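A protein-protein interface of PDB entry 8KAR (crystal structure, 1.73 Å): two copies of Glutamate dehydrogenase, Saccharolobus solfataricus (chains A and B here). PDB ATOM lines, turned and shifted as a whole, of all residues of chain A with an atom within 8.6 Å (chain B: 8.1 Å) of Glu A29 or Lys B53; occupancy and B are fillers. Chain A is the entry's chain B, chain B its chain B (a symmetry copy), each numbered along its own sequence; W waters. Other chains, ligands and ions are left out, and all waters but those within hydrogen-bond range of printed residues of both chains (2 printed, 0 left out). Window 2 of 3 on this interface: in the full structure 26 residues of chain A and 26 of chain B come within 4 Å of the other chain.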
ATOM      1  N   TYR A  18       0.464  15.424  -7.749  1.00  0.00           N
ATOM      2  CA  TYR A  18      -0.250  16.662  -7.420  1.00  0.00           C
ATOM      3  C   TYR A  18      -1.763  16.511  -7.609  1.00  0.00           C
ATOM      4  O   TYR A  18      -2.527  17.131  -6.866  1.00  0.00           O
ATOM      5  CB  TYR A  18       0.284  17.894  -8.167  1.00  0.00           C
ATOM      6  CG  TYR A  18       1.523  18.479  -7.530  1.00  0.00           C
ATOM      7  CD1 TYR A  18       2.764  17.918  -7.778  1.00  0.00           C
ATOM      8  CD2 TYR A  18       1.458  19.510  -6.603  1.00  0.00           C
ATOM      9  CE1 TYR A  18       3.916  18.396  -7.177  1.00  0.00           C
ATOM     10  CE2 TYR A  18       2.600  20.003  -5.987  1.00  0.00           C
ATOM     11  CZ  TYR A  18       3.835  19.437  -6.274  1.00  0.00           C
ATOM     12  OH  TYR A  18       5.005  19.841  -5.687  1.00  0.00           O
ATOM     13  N   LEU A  26      -4.830  17.923   0.224  1.00  0.00           N
ATOM     14  CA  LEU A  26      -3.537  18.207   0.818  1.00  0.00           C
ATOM     15  C   LEU A  26      -3.050  19.587   0.400  1.00  0.00           C
ATOM     16  O   LEU A  26      -3.189  19.959  -0.762  1.00  0.00           O
ATOM     17  CB  LEU A  26      -2.526  17.157   0.336  1.00  0.00           C
ATOM     18  CG  LEU A  26      -2.815  15.718   0.754  1.00  0.00           C
ATOM     19  CD1 LEU A  26      -1.675  14.817   0.312  1.00  0.00           C
ATOM     20  CD2 LEU A  26      -3.030  15.620   2.252  1.00  0.00           C
ATOM     21  N   ASP A  27      -2.387  20.271   1.344  1.00  0.00           N
ATOM     22  CA  ASP A  27      -1.640  21.479   1.045  1.00  0.00           C
ATOM     23  C   ASP A  27      -0.638  21.199  -0.064  1.00  0.00           C
ATOM     24  O   ASP A  27       0.030  20.157  -0.063  1.00  0.00           O
ATOM     25  CB  ASP A  27      -0.775  21.936   2.224  1.00  0.00           C
ATOM     26  CG  ASP A  27      -1.518  22.345   3.479  1.00  0.00           C
ATOM     27  OD1 ASP A  27      -2.735  22.662   3.395  1.00  0.00           O
ATOM     28  OD2 ASP A  27      -0.870  22.331   4.545  1.00  0.00           O
ATOM     29  N   SER A  28      -0.475  22.185  -0.936  1.00  0.00           N
ATOM     30  CA  SER A  28       0.588  22.190  -1.918  1.00  0.00           C
ATOM     31  C   SER A  28       1.955  21.876  -1.275  1.00  0.00           C
ATOM     32  O   SER A  28       2.821  21.240  -1.877  1.00  0.00           O
ATOM     33  CB  SER A  28       0.571  23.520  -2.592  1.00  0.00           C
ATOM     34  OG  SER A  28       1.552  23.571  -3.600  1.00  0.00           O
ATOM     35  N   GLU A  29       2.147  22.302  -0.025  1.00  0.00           N
ATOM     36  CA  GLU A  29       3.445  22.216   0.618  1.00  0.00           C
ATOM     37  C   GLU A  29       3.724  20.773   1.034  1.00  0.00           C
ATOM     38  O   GLU A  29       4.874  20.327   0.972  1.00  0.00           O
ATOM     39  CB  GLU A  29       3.500  23.157   1.826  1.00  0.00           C
ATOM     40  CG  GLU A  29       3.552  24.627   1.456  1.00  0.00           C
ATOM     41  CD  GLU A  29       2.216  25.322   1.212  1.00  0.00           C
ATOM     42  OE1 GLU A  29       2.230  26.552   1.105  1.00  0.00           O
ATOM     43  OE2 GLU A  29       1.185  24.648   1.103  1.00  0.00           O
ATOM     44  N   THR A  30       2.647  20.052   1.412  1.00  0.00           N
ATOM     45  CA  THR A  30       2.727  18.642   1.741  1.00  0.00           C
ATOM     46  C   THR A  30       3.140  17.837   0.502  1.00  0.00           C
ATOM     47  O   THR A  30       3.967  16.942   0.583  1.00  0.00           O
ATOM     48  CB  THR A  30       1.390  18.123   2.293  1.00  0.00           C
ATOM     49  OG1 THR A  30       0.950  18.939   3.379  1.00  0.00           O
ATOM     50  CG2 THR A  30       1.464  16.686   2.751  1.00  0.00           C
ATOM     51  N   ILE A  31       2.519  18.128  -0.639  1.00  0.00           N
ATOM     52  CA  ILE A  31       2.786  17.432  -1.895  1.00  0.00           C
ATOM     53  C   ILE A  31       4.232  17.662  -2.319  1.00  0.00           C
ATOM     54  O   ILE A  31       4.880  16.713  -2.750  1.00  0.00           O
ATOM     55  CB  ILE A  31       1.790  17.833  -2.999  1.00  0.00           C
ATOM     56  CG1 ILE A  31       0.336  17.640  -2.556  1.00  0.00           C
ATOM     57  CG2 ILE A  31       2.085  17.043  -4.263  1.00  0.00           C
ATOM     58  CD1 ILE A  31      -0.671  18.471  -3.329  1.00  0.00           C
ATOM     59  N   ASP A  32       4.764  18.875  -2.085  1.00  0.00           N
ATOM     60  CA  ASP A  32       6.158  19.183  -2.383  1.00  0.00           C
ATOM     61  C   ASP A  32       7.085  18.200  -1.674  1.00  0.00           C
ATOM     62  O   ASP A  32       8.092  17.737  -2.227  1.00  0.00           O
ATOM     63  CB  ASP A  32       6.537  20.603  -1.931  1.00  0.00           C
ATOM     64  CG  ASP A  32       5.859  21.741  -2.699  1.00  0.00           C
ATOM     65  OD1 ASP A  32       5.440  21.507  -3.834  1.00  0.00           O
ATOM     66  OD2 ASP A  32       5.735  22.856  -2.139  1.00  0.00           O
ATOM     67  N   VAL A  33       6.756  17.900  -0.410  1.00  0.00           N
ATOM     68  CA  VAL A  33       7.562  16.951   0.336  1.00  0.00           C
ATOM     69  C   VAL A  33       7.490  15.575  -0.314  1.00  0.00           C
ATOM     70  O   VAL A  33       8.515  14.898  -0.412  1.00  0.00           O
ATOM     71  CB  VAL A  33       7.160  16.862   1.822  1.00  0.00           C
ATOM     72  CG1 VAL A  33       7.965  15.794   2.539  1.00  0.00           C
ATOM     73  CG2 VAL A  33       7.275  18.202   2.549  1.00  0.00           C
ATOM     74  N   LEU A  34       6.273  15.067  -0.565  1.00  0.00           N
ATOM     75  CA  LEU A  34       6.127  13.741  -1.147  1.00  0.00           C
ATOM     76  C   LEU A  34       6.760  13.629  -2.538  1.00  0.00           C
ATOM     77  O   LEU A  34       7.158  12.528  -2.930  1.00  0.00           O
ATOM     78  CB  LEU A  34       4.644  13.378  -1.248  1.00  0.00           C
ATOM     79  CG  LEU A  34       3.853  13.367   0.052  1.00  0.00           C
ATOM     80  CD1 LEU A  34       2.357  13.222  -0.246  1.00  0.00           C
ATOM     81  CD2 LEU A  34       4.363  12.277   0.949  1.00  0.00           C
ATOM     82  N   SER A  35       6.767  14.718  -3.311  1.00  0.00           N
ATOM     83  CA  SER A  35       7.218  14.691  -4.700  1.00  0.00           C
ATOM     84  C   SER A  35       8.750  14.655  -4.867  1.00  0.00           C
ATOM     85  O   SER A  35       9.247  14.685  -6.009  1.00  0.00           O
ATOM     86  CB  SER A  35       6.659  15.871  -5.430  1.00  0.00           C
ATOM     87  OG  SER A  35       7.406  17.054  -5.106  1.00  0.00           O
ATOM     88  N   LEU A 418       6.938  14.652  10.752  1.00  0.00           N
ATOM     89  CA  LEU A 418       7.778  14.991   9.615  1.00  0.00           C
ATOM     90  C   LEU A 418       7.069  15.944   8.653  1.00  0.00           C
ATOM     91  O   LEU A 418       7.703  16.423   7.723  1.00  0.00           O
ATOM     92  CB  LEU A 418       8.153  13.713   8.899  1.00  0.00           C
ATOM     93  CG  LEU A 418       9.052  12.785   9.700  1.00  0.00           C
ATOM     94  CD1 LEU A 418       9.238  11.505   8.965  1.00  0.00           C
ATOM     95  CD2 LEU A 418      10.398  13.453   9.983  1.00  0.00           C
ATOM     96  N   LEU A 419       5.814  16.263   8.979  1.00  0.00           N
ATOM     97  CA  LEU A 419       4.864  16.863   8.062  1.00  0.00           C
ATOM     98  C   LEU A 419       3.814  17.571   8.913  1.00  0.00           C
ATOM     99  O   LEU A 419       3.606  18.778   8.671  1.00  0.00           O
ATOM    100  CB  LEU A 419       4.240  15.709   7.272  1.00  0.00           C
ATOM    101  CG  LEU A 419       3.878  15.962   5.823  1.00  0.00           C
ATOM    102  CD1 LEU A 419       5.123  16.154   4.983  1.00  0.00           C
ATOM    103  CD2 LEU A 419       3.041  14.812   5.299  1.00  0.00           C
ATOM    104  OXT LEU A 419       3.290  16.882   9.838  1.00  0.00           O
ATOM    105  N   GLN B  46      12.873  19.284   4.765  1.00  0.00           N
ATOM    106  CA  GLN B  46      11.663  20.078   4.990  1.00  0.00           C
ATOM    107  C   GLN B  46      11.725  20.728   6.376  1.00  0.00           C
ATOM    108  O   GLN B  46      12.207  20.122   7.331  1.00  0.00           O
ATOM    109  CB  GLN B  46      10.363  19.279   4.773  1.00  0.00           C
ATOM    110  CG  GLN B  46      10.086  18.163   5.778  1.00  0.00           C
ATOM    111  CD  GLN B  46      10.436  16.766   5.296  1.00  0.00           C
ATOM    112  OE1 GLN B  46      11.150  16.574   4.314  1.00  0.00           O
ATOM    113  NE2 GLN B  46       9.904  15.764   5.981  1.00  0.00           N
ATOM    114  N   ILE B  47      11.217  21.969   6.444  1.00  0.00           N
ATOM    115  CA  ILE B  47      11.284  22.834   7.610  1.00  0.00           C
ATOM    116  C   ILE B  47       9.929  23.514   7.790  1.00  0.00           C
ATOM    117  O   ILE B  47       9.382  24.045   6.834  1.00  0.00           O
ATOM    118  CB  ILE B  47      12.422  23.865   7.428  1.00  0.00           C
ATOM    119  CG1 ILE B  47      13.791  23.175   7.399  1.00  0.00           C
ATOM    120  CG2 ILE B  47      12.367  24.952   8.486  1.00  0.00           C
ATOM    121  CD1 ILE B  47      14.945  24.117   7.217  1.00  0.00           C
ATOM    122  N   ARG B  48       9.414  23.479   9.026  1.00  0.00           N
ATOM    123  CA  ARG B  48       8.225  24.223   9.420  1.00  0.00           C
ATOM    124  C   ARG B  48       8.699  25.603   9.860  1.00  0.00           C
ATOM    125  O   ARG B  48       9.454  25.712  10.814  1.00  0.00           O
ATOM    126  CB  ARG B  48       7.481  23.449  10.514  1.00  0.00           C
ATOM    127  CG  ARG B  48       6.231  24.127  11.063  1.00  0.00           C
ATOM    128  CD  ARG B  48       5.066  24.143  10.096  1.00  0.00           C
ATOM    129  NE  ARG B  48       4.548  22.817   9.779  1.00  0.00           N
ATOM    130  CZ  ARG B  48       3.625  22.584   8.851  1.00  0.00           C
ATOM    131  NH1 ARG B  48       3.198  23.567   8.074  1.00  0.00           N
ATOM    132  NH2 ARG B  48       3.136  21.371   8.691  1.00  0.00           N
ATOM    133  N   SER B  49       8.316  26.639   9.114  1.00  0.00           N
ATOM    134  CA  SER B  49       8.880  27.969   9.284  1.00  0.00           C
ATOM    135  C   SER B  49       8.142  28.708  10.406  1.00  0.00           C
ATOM    136  O   SER B  49       7.161  28.188  10.943  1.00  0.00           O
ATOM    137  CB  SER B  49       8.851  28.697   7.958  1.00  0.00           C
ATOM    138  OG  SER B  49       9.458  27.895   6.941  1.00  0.00           O
ATOM    139  N   SER B  50       8.640  29.899  10.783  1.00  0.00           N
ATOM    140  CA  SER B  50       8.075  30.663  11.895  1.00  0.00           C
ATOM    141  C   SER B  50       6.664  31.167  11.572  1.00  0.00           C
ATOM    142  O   SER B  50       5.840  31.265  12.472  1.00  0.00           O
ATOM    143  CB  SER B  50       8.995  31.788  12.347  1.00  0.00           C
ATOM    144  OG  SER B  50       9.673  32.393  11.254  1.00  0.00           O
ATOM    145  N   ASP B  51       6.375  31.440  10.290  1.00  0.00           N
ATOM    146  CA  ASP B  51       5.029  31.771   9.831  1.00  0.00           C
ATOM    147  C   ASP B  51       4.066  30.588   9.994  1.00  0.00           C
ATOM    148  O   ASP B  51       2.866  30.806  10.102  1.00  0.00           O
ATOM    149  CB  ASP B  51       5.030  32.313   8.391  1.00  0.00           C
ATOM    150  CG  ASP B  51       5.841  31.544   7.349  1.00  0.00           C
ATOM    151  OD1 ASP B  51       6.258  30.393   7.624  1.00  0.00           O
ATOM    152  OD2 ASP B  51       6.070  32.112   6.261  1.00  0.00           O
ATOM    153  N   GLY B  52       4.566  29.343  10.021  1.00  0.00           N
ATOM    154  CA  GLY B  52       3.718  28.155  10.092  1.00  0.00           C
ATOM    155  C   GLY B  52       3.720  27.344   8.790  1.00  0.00           C
ATOM    156  O   GLY B  52       3.167  26.255   8.724  1.00  0.00           O
ATOM    157  N   LYS B  53       4.367  27.879   7.756  1.00  0.00           N
ATOM    158  CA  LYS B  53       4.420  27.257   6.445  1.00  0.00           C
ATOM    159  C   LYS B  53       5.503  26.172   6.422  1.00  0.00           C
ATOM    160  O   LYS B  53       6.592  26.355   6.949  1.00  0.00           O
ATOM    161  CB  LYS B  53       4.706  28.358   5.421  1.00  0.00           C
ATOM    162  CG  LYS B  53       4.897  27.910   3.977  1.00  0.00           C
ATOM    163  CD  LYS B  53       3.901  28.498   2.997  1.00  0.00           C
ATOM    164  CE  LYS B  53       4.390  28.398   1.564  1.00  0.00           C
ATOM    165  NZ  LYS B  53       5.675  29.108   1.384  1.00  0.00           N
ATOM    166  N   LEU B  54       5.204  25.048   5.774  1.00  0.00           N
ATOM    167  CA  LEU B  54       6.203  24.010   5.518  1.00  0.00           C
ATOM    168  C   LEU B  54       6.936  24.328   4.211  1.00  0.00           C
ATOM    169  O   LEU B  54       6.293  24.660   3.228  1.00  0.00           O
ATOM    170  CB  LEU B  54       5.453  22.676   5.458  1.00  0.00           C
ATOM    171  CG  LEU B  54       6.282  21.405   5.291  1.00  0.00           C
ATOM    172  CD1 LEU B  54       7.227  21.206   6.456  1.00  0.00           C
ATOM    173  CD2 LEU B  54       5.359  20.196   5.156  1.00  0.00           C
ATOM    174  N   ARG B  55       8.279  24.278   4.211  1.00  0.00           N
ATOM    175  CA  ARG B  55       9.081  24.534   3.021  1.00  0.00           C
ATOM    176  C   ARG B  55      10.065  23.382   2.803  1.00  0.00           C
ATOM    177  O   ARG B  55      10.573  22.827   3.761  1.00  0.00           O
ATOM    178  CB  ARG B  55       9.789  25.889   3.158  1.00  0.00           C
ATOM    179  CG  ARG B  55       8.817  27.066   3.025  1.00  0.00           C
ATOM    180  CD  ARG B  55       9.440  28.458   3.060  1.00  0.00           C
ATOM    181  NE  ARG B  55      10.074  28.706   4.353  1.00  0.00           N
ATOM    182  CZ  ARG B  55      10.762  29.801   4.682  1.00  0.00           C
ATOM    183  NH1 ARG B  55      11.312  29.899   5.884  1.00  0.00           N
ATOM    184  NH2 ARG B  55      10.900  30.796   3.818  1.00  0.00           N
ATOM    185  N   THR B  56      10.309  23.035   1.533  1.00  0.00           N
ATOM    186  CA  THR B  56      11.218  21.945   1.209  1.00  0.00           C
ATOM    187  C   THR B  56      12.418  22.488   0.457  1.00  0.00           C
ATOM    188  O   THR B  56      12.247  23.234  -0.514  1.00  0.00           O
ATOM    189  CB  THR B  56      10.556  20.874   0.344  1.00  0.00           C
ATOM    190  OG1 THR B  56       9.363  20.410   0.962  1.00  0.00           O
ATOM    191  CG2 THR B  56      11.505  19.718   0.086  1.00  0.00           C
ATOM    192  N   PHE B  57      13.614  22.013   0.835  1.00  0.00           N
ATOM    193  CA  PHE B  57      14.839  22.464   0.213  1.00  0.00           C
ATOM    194  C   PHE B  57      15.645  21.246  -0.231  1.00  0.00           C
ATOM    195  O   PHE B  57      15.671  20.219   0.470  1.00  0.00           O
ATOM    196  CB  PHE B  57      15.626  23.348   1.175  1.00  0.00           C
ATOM    197  CG  PHE B  57      14.875  24.565   1.670  1.00  0.00           C
ATOM    198  CD1 PHE B  57      14.807  25.713   0.902  1.00  0.00           C
ATOM    199  CD2 PHE B  57      14.235  24.553   2.904  1.00  0.00           C
ATOM    200  CE1 PHE B  57      14.120  26.834   1.355  1.00  0.00           C
ATOM    201  CE2 PHE B  57      13.537  25.670   3.340  1.00  0.00           C
ATOM    202  CZ  PHE B  57      13.517  26.806   2.589  1.00  0.00           C
ATOM    203  N   GLU B 122      15.546  28.636  11.784  1.00  0.00           N
ATOM    204  CA  GLU B 122      15.322  27.936  10.527  1.00  0.00           C
ATOM    205  C   GLU B 122      16.641  27.497   9.883  1.00  0.00           C
ATOM    206  O   GLU B 122      16.717  26.441   9.269  1.00  0.00           O
ATOM    207  CB  GLU B 122      14.530  28.824   9.562  1.00  0.00           C
ATOM    208  CG  GLU B 122      13.079  29.015   9.968  1.00  0.00           C
ATOM    209  CD  GLU B 122      12.322  30.145   9.261  1.00  0.00           C
ATOM    210  OE1 GLU B 122      12.948  30.978   8.620  1.00  0.00           O
ATOM    211  OE2 GLU B 122      11.091  30.207   9.429  1.00  0.00           O
HETATM  212  O   HOH W   1       7.059  21.987   1.453  1.00  0.00           O
HETATM  213  O   HOH W   2       8.509  24.007  -0.600  1.00  0.00           O
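The chain-end carboxylate (O) of Leu A419 lies within salt-bridge range of the guanidinium group (NH2) of Arg B48, 2.6 Å away. NE2 of Gln B46 is in hydrogen-bond range of O of Leu A418.
Water W1 lies within hydrogen-bond range of the backbone carbonyl oxygen (O) of Glu A29 (2.8 Å), the side-chain hydroxyl (OG1) of Thr B56 (2.8 Å) and the backbone carbonyl oxygen (O) of Leu B54 (3.3 Å). Water W2 bridges the backbone NH of Thr B56 (3.0 Å) and the side-chain carboxylate of Asp A32 (3.4 Å).
No position is printed for both chains. Of the 7 pairs that touch across the chains among the printed residues, none has its exchanged pair printed and touching as well.
Of the 13 printed residues of chain B, 5 touch a printed residue of chain A. Of the 13 printed residues of chain A, 4 touch a printed residue of chain B. Hydrophobic or aromatic side chains of chain A that line the printed part of chain B: Val A33 and Leu A418. Among the printed residues, no Asp or Glu carboxylate lies within 4 Å of a Lys or Arg side-chain nitrogen of the other chain.
Among the printed residues, pairs that only touch across the chains: Glu A29 with Lys B53, Glu A29 with Leu B54, Val A33 with Thr B56, Val A33 with Gln B46 and Val A33 with Leu B54.
Asp A27 touches none of the printed residues of chain B. Ser A28 touches none of the printed residues of chain B. Glu A29 touches two residues of chain B. Ser A35 touches none of the printed residues of chain B. Printed residues of chain B within 4 Å of Leu A418: Gln B46 (2.9 Å). Of the printed residues of chain B, Leu A419 touches Arg B48. Of the printed residues of chain A, Gln B46 touches Val A33 and Leu A418. Printed residues of chain A within 4 Å of Lys B53: Glu A29 (2.9 Å). Printed residues of chain A within 4 Å of Leu B54: Glu A29 (3.3 Å) and Val A33 (3.8 Å).
The side-chain carboxylate (OD1) of Asp B51 is in hydrogen-bond range of the backbone NH (N) of Lys B53, at 3.1 Å. The guanidinium group (NH1) of Arg B48 is in hydrogen-bond range of the backbone carbonyl oxygen (O) of Gly B52 (2.8 Å). O of Lys B53 sits at hydrogen-bond distance from OG of Ser B49 (3.3 Å).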
